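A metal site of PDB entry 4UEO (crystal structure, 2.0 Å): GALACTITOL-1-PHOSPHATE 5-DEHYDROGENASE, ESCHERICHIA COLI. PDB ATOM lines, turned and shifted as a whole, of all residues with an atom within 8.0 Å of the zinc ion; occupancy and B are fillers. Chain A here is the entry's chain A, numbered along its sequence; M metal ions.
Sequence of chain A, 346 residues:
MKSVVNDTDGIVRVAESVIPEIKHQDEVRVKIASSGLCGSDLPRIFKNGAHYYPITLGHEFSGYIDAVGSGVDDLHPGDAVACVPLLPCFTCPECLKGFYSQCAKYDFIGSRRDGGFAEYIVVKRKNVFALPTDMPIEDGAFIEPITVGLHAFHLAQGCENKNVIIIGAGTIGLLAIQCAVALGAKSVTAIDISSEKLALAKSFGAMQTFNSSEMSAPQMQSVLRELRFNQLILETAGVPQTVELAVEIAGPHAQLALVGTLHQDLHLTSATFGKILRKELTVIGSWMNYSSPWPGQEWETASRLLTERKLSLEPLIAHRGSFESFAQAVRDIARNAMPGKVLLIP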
ATOM      1  N   LEU A  87     -12.967  27.050 -32.925  1.00  0.00           N
ATOM      2  CA  LEU A  87     -12.486  25.851 -32.233  1.00  0.00           C
ATOM      3  C   LEU A  87     -10.995  25.975 -31.940  1.00  0.00           C
ATOM      4  O   LEU A  87     -10.165  25.736 -32.816  1.00  0.00           O
ATOM      5  CB  LEU A  87     -12.753  24.576 -33.058  1.00  0.00           C
ATOM      6  CG  LEU A  87     -12.489  23.198 -32.406  1.00  0.00           C
ATOM      7  CD1 LEU A  87     -13.618  22.735 -31.452  1.00  0.00           C
ATOM      8  CD2 LEU A  87     -12.203  22.143 -33.463  1.00  0.00           C
ATOM      9  N   PRO A  88     -10.642  26.399 -30.710  1.00  0.00           N
ATOM     10  CA  PRO A  88      -9.234  26.434 -30.287  1.00  0.00           C
ATOM     11  C   PRO A  88      -8.727  25.026 -30.036  1.00  0.00           C
ATOM     12  O   PRO A  88      -9.523  24.102 -29.917  1.00  0.00           O
ATOM     13  CB  PRO A  88      -9.256  27.251 -29.003  1.00  0.00           C
ATOM     14  CG  PRO A  88     -10.620  27.054 -28.467  1.00  0.00           C
ATOM     15  CD  PRO A  88     -11.550  26.846 -29.643  1.00  0.00           C
ATOM     16  N   CYS A  89      -7.409  24.857 -29.934  1.00  0.00           N
ATOM     17  CA  CYS A  89      -6.865  23.509 -29.833  1.00  0.00           C
ATOM     18  C   CYS A  89      -7.004  22.975 -28.405  1.00  0.00           C
ATOM     19  O   CYS A  89      -7.000  21.770 -28.201  1.00  0.00           O
ATOM     20  CB  CYS A  89      -5.417  23.506 -30.281  1.00  0.00           C
ATOM     21  SG  CYS A  89      -4.240  23.994 -29.025  1.00  0.00           S
ATOM     22  N   PHE A  90      -7.149  23.900 -27.450  1.00  0.00           N
ATOM     23  CA  PHE A  90      -7.261  23.624 -26.011  1.00  0.00           C
ATOM     24  C   PHE A  90      -6.040  22.977 -25.320  1.00  0.00           C
ATOM     25  O   PHE A  90      -6.128  22.578 -24.162  1.00  0.00           O
ATOM     26  CB  PHE A  90      -8.499  22.754 -25.729  1.00  0.00           C
ATOM     27  CG  PHE A  90      -9.810  23.423 -26.089  1.00  0.00           C
ATOM     28  CD1 PHE A  90     -10.281  24.493 -25.351  1.00  0.00           C
ATOM     29  CD2 PHE A  90     -10.578  22.951 -27.147  1.00  0.00           C
ATOM     30  CE1 PHE A  90     -11.478  25.099 -25.662  1.00  0.00           C
ATOM     31  CE2 PHE A  90     -11.776  23.557 -27.468  1.00  0.00           C
ATOM     32  CZ  PHE A  90     -12.233  24.629 -26.720  1.00  0.00           C
ATOM     33  N   THR A  91      -4.901  22.892 -25.996  1.00  0.00           N
ATOM     34  CA  THR A  91      -3.740  22.263 -25.355  1.00  0.00           C
ATOM     35  C   THR A  91      -2.468  23.109 -25.358  1.00  0.00           C
ATOM     36  O   THR A  91      -1.548  22.856 -24.554  1.00  0.00           O
ATOM     37  CB  THR A  91      -3.397  20.893 -26.014  1.00  0.00           C
ATOM     38  OG1 THR A  91      -3.254  21.052 -27.424  1.00  0.00           O
ATOM     39  CG2 THR A  91      -4.490  19.879 -25.733  1.00  0.00           C
ATOM     40  N   CYS A  92      -2.409  24.092 -26.244  1.00  0.00           N
ATOM     41  CA  CYS A  92      -1.225  24.950 -26.315  1.00  0.00           C
ATOM     42  C   CYS A  92      -1.164  25.857 -25.071  1.00  0.00           C
ATOM     43  O   CYS A  92      -2.167  26.019 -24.385  1.00  0.00           O
ATOM     44  CB  CYS A  92      -1.252  25.775 -27.591  1.00  0.00           C
ATOM     45  SG  CYS A  92      -2.525  27.055 -27.559  1.00  0.00           S
ATOM     46  N   PRO A  93       0.022  26.424 -24.775  1.00  0.00           N
ATOM     47  CA  PRO A  93       0.163  27.326 -23.621  1.00  0.00           C
ATOM     48  C   PRO A  93      -0.882  28.443 -23.570  1.00  0.00           C
ATOM     49  O   PRO A  93      -1.445  28.684 -22.496  1.00  0.00           O
ATOM     50  CB  PRO A  93       1.568  27.904 -23.806  1.00  0.00           C
ATOM     51  CG  PRO A  93       2.315  26.759 -24.405  1.00  0.00           C
ATOM     52  CD  PRO A  93       1.339  26.136 -25.383  1.00  0.00           C
ATOM     53  N   GLU A  94      -1.152  29.116 -24.686  1.00  0.00           N
ATOM     54  CA  GLU A  94      -2.198  30.126 -24.705  1.00  0.00           C
ATOM     55  C   GLU A  94      -3.504  29.529 -24.202  1.00  0.00           C
ATOM     56  O   GLU A  94      -4.124  30.085 -23.306  1.00  0.00           O
ATOM     57  CB  GLU A  94      -2.419  30.695 -26.112  1.00  0.00           C
ATOM     58  CG  GLU A  94      -1.445  31.766 -26.561  1.00  0.00           C
ATOM     59  CD  GLU A  94      -0.055  31.224 -26.881  1.00  0.00           C
ATOM     60  OE1 GLU A  94       0.185  29.995 -26.828  1.00  0.00           O
ATOM     61  OE2 GLU A  94       0.831  32.053 -27.172  1.00  0.00           O
ATOM     62  N   CYS A  95      -3.898  28.386 -24.765  1.00  0.00           N
ATOM     63  CA  CYS A  95      -5.225  27.852 -24.471  1.00  0.00           C
ATOM     64  C   CYS A  95      -5.389  27.479 -23.012  1.00  0.00           C
ATOM     65  O   CYS A  95      -6.445  27.689 -22.415  1.00  0.00           O
ATOM     66  CB  CYS A  95      -5.512  26.639 -25.345  1.00  0.00           C
ATOM     67  SG  CYS A  95      -6.274  27.065 -26.889  1.00  0.00           S
ATOM     68  N   LEU A  96      -4.321  26.947 -22.450  1.00  0.00           N
ATOM     69  CA  LEU A  96      -4.297  26.604 -21.042  1.00  0.00           C
ATOM     70  C   LEU A  96      -4.509  27.826 -20.144  1.00  0.00           C
ATOM     71  O   LEU A  96      -4.922  27.679 -19.003  1.00  0.00           O
ATOM     72  CB  LEU A  96      -2.983  25.921 -20.692  1.00  0.00           C
ATOM     73  CG  LEU A  96      -2.825  24.543 -21.329  1.00  0.00           C
ATOM     74  CD1 LEU A  96      -1.571  23.839 -20.809  1.00  0.00           C
ATOM     75  CD2 LEU A  96      -4.077  23.706 -21.087  1.00  0.00           C
ATOM     76  N   PHE A  99      -6.507  32.008 -23.204  1.00  0.00           N
ATOM     77  CA  PHE A  99      -6.332  32.915 -24.331  1.00  0.00           C
ATOM     78  C   PHE A  99      -6.730  32.209 -25.632  1.00  0.00           C
ATOM     79  O   PHE A  99      -5.936  32.150 -26.576  1.00  0.00           O
ATOM     80  CB  PHE A  99      -4.888  33.407 -24.416  1.00  0.00           C
ATOM     81  CG  PHE A  99      -4.425  34.178 -23.204  1.00  0.00           C
ATOM     82  CD1 PHE A  99      -5.316  34.795 -22.357  1.00  0.00           C
ATOM     83  CD2 PHE A  99      -3.067  34.283 -22.931  1.00  0.00           C
ATOM     84  CE1 PHE A  99      -4.870  35.505 -21.236  1.00  0.00           C
ATOM     85  CE2 PHE A  99      -2.612  34.988 -21.820  1.00  0.00           C
ATOM     86  CZ  PHE A  99      -3.518  35.602 -20.972  1.00  0.00           C
ATOM     87  N   TYR A 100      -7.945  31.684 -25.678  1.00  0.00           N
ATOM     88  CA  TYR A 100      -8.430  30.916 -26.839  1.00  0.00           C
ATOM     89  C   TYR A 100      -8.288  31.652 -28.157  1.00  0.00           C
ATOM     90  O   TYR A 100      -7.921  31.060 -29.161  1.00  0.00           O
ATOM     91  CB  TYR A 100      -9.883  30.537 -26.644  1.00  0.00           C
ATOM     92  CG  TYR A 100     -10.114  29.849 -25.336  1.00  0.00           C
ATOM     93  CD1 TYR A 100      -9.583  28.605 -25.085  1.00  0.00           C
ATOM     94  CD2 TYR A 100     -10.858  30.451 -24.349  1.00  0.00           C
ATOM     95  CE1 TYR A 100      -9.781  27.967 -23.877  1.00  0.00           C
ATOM     96  CE2 TYR A 100     -11.079  29.815 -23.131  1.00  0.00           C
ATOM     97  CZ  TYR A 100     -10.528  28.583 -22.910  1.00  0.00           C
ATOM     98  OH  TYR A 100     -10.721  27.953 -21.702  1.00  0.00           O
ATOM     99  N   SER A 101      -8.554  32.947 -28.149  1.00  0.00           N
ATOM    100  CA  SER A 101      -8.433  33.757 -29.346  1.00  0.00           C
ATOM    101  C   SER A 101      -6.985  33.970 -29.752  1.00  0.00           C
ATOM    102  O   SER A 101      -6.711  34.486 -30.841  1.00  0.00           O
ATOM    103  CB  SER A 101      -9.129  35.109 -29.146  1.00  0.00           C
ATOM    104  OG  SER A 101     -10.495  34.913 -28.820  1.00  0.00           O
ATOM    105  N   GLN A 102      -6.057  33.603 -28.869  1.00  0.00           N
ATOM    106  CA  GLN A 102      -4.647  33.650 -29.226  1.00  0.00           C
ATOM    107  C   GLN A 102      -4.110  32.259 -29.535  1.00  0.00           C
ATOM    108  O   GLN A 102      -2.898  32.077 -29.682  1.00  0.00           O
ATOM    109  CB  GLN A 102      -3.801  34.310 -28.117  1.00  0.00           C
ATOM    110  CG  GLN A 102      -3.912  35.838 -28.029  1.00  0.00           C
ATOM    111  CD  GLN A 102      -5.277  36.290 -27.530  1.00  0.00           C
ATOM    112  OE1 GLN A 102      -5.804  35.739 -26.560  1.00  0.00           O
ATOM    113  NE2 GLN A 102      -5.872  37.264 -28.202  1.00  0.00           N
ATOM    114  N   CYS A 103      -4.995  31.274 -29.606  1.00  0.00           N
ATOM    115  CA  CYS A 103      -4.572  29.948 -30.044  1.00  0.00           C
ATOM    116  C   CYS A 103      -4.077  30.077 -31.476  1.00  0.00           C
ATOM    117  O   CYS A 103      -4.708  30.763 -32.260  1.00  0.00           O
ATOM    118  CB  CYS A 103      -5.716  28.932 -29.943  1.00  0.00           C
ATOM    119  SG  CYS A 103      -5.261  27.260 -30.444  1.00  0.00           S
ATOM    120  N   ALA A 104      -2.958  29.453 -31.815  1.00  0.00           N
ATOM    121  CA  ALA A 104      -2.380  29.598 -33.157  1.00  0.00           C
ATOM    122  C   ALA A 104      -2.934  28.562 -34.139  1.00  0.00           C
ATOM    123  O   ALA A 104      -2.835  28.726 -35.359  1.00  0.00           O
ATOM    124  CB  ALA A 104      -0.854  29.507 -33.086  1.00  0.00           C
ATOM    125  N   LYS A 105      -3.516  27.484 -33.612  1.00  0.00           N
ATOM    126  CA  LYS A 105      -4.047  26.408 -34.444  1.00  0.00           C
ATOM    127  C   LYS A 105      -5.555  26.271 -34.247  1.00  0.00           C
ATOM    128  O   LYS A 105      -6.043  25.226 -33.809  1.00  0.00           O
ATOM    129  CB  LYS A 105      -3.362  25.087 -34.134  1.00  0.00           C
ATOM    130  CG  LYS A 105      -1.866  25.064 -34.412  1.00  0.00           C
ATOM    131  CD  LYS A 105      -1.165  24.139 -33.430  1.00  0.00           C
ATOM    132  CE  LYS A 105      -1.757  24.315 -32.026  1.00  0.00           C
ATOM    133  NZ  LYS A 105      -1.305  23.267 -31.083  1.00  0.00           N
ATOM    134  N   TYR A 106      -6.256  27.351 -34.568  1.00  0.00           N
ATOM    135  CA  TYR A 106      -7.703  27.486 -34.470  1.00  0.00           C
ATOM    136  C   TYR A 106      -8.433  26.820 -35.629  1.00  0.00           C
ATOM    137  O   TYR A 106      -7.936  26.804 -36.752  1.00  0.00           O
ATOM    138  CB  TYR A 106      -8.045  28.975 -34.441  1.00  0.00           C
ATOM    139  CG  TYR A 106      -7.081  29.765 -35.302  1.00  0.00           C
ATOM    140  CD1 TYR A 106      -7.216  29.796 -36.691  1.00  0.00           C
ATOM    141  CD2 TYR A 106      -6.019  30.450 -34.734  1.00  0.00           C
ATOM    142  CE1 TYR A 106      -6.308  30.502 -37.483  1.00  0.00           C
ATOM    143  CE2 TYR A 106      -5.117  31.148 -35.516  1.00  0.00           C
ATOM    144  CZ  TYR A 106      -5.265  31.176 -36.885  1.00  0.00           C
ATOM    145  OH  TYR A 106      -4.357  31.882 -37.646  1.00  0.00           O
HETATM  146 ZN    ZN M   1      -4.559  26.285 -28.402  1.00  0.00          ZN
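SG of Cys 92 sits close to N of Glu 94.
N of Lys 105 sits close to SG of Cys 103.
The side-chain sulfur (SG) of Cys 89 lies close to the backbone NH (N) of Thr 91.
The side-chain sulfur of Cys 89 sits close to the side-chain amino group of Lys 105 (3.7 Å).
SG of Cys 95 lies close to N of Phe 90.
Merely in contact with the zinc ion: Phe 90.
Within 4 Å of the zinc ion: Cys 89, Phe 90, Cys 92, Cys 95 and Cys 103.
The nearest printed residue that does not touch the zinc ion is Thr 91 (4.2 Å).
The zinc ion is bound by the side-chain sulfur of Cys 92 (2.3 Å), the side-chain sulfur of Cys 103 (2.4 Å), the side-chain sulfur of Cys 89 (2.4 Å) and the side-chain sulfur of Cys 95 (2.4 Å).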
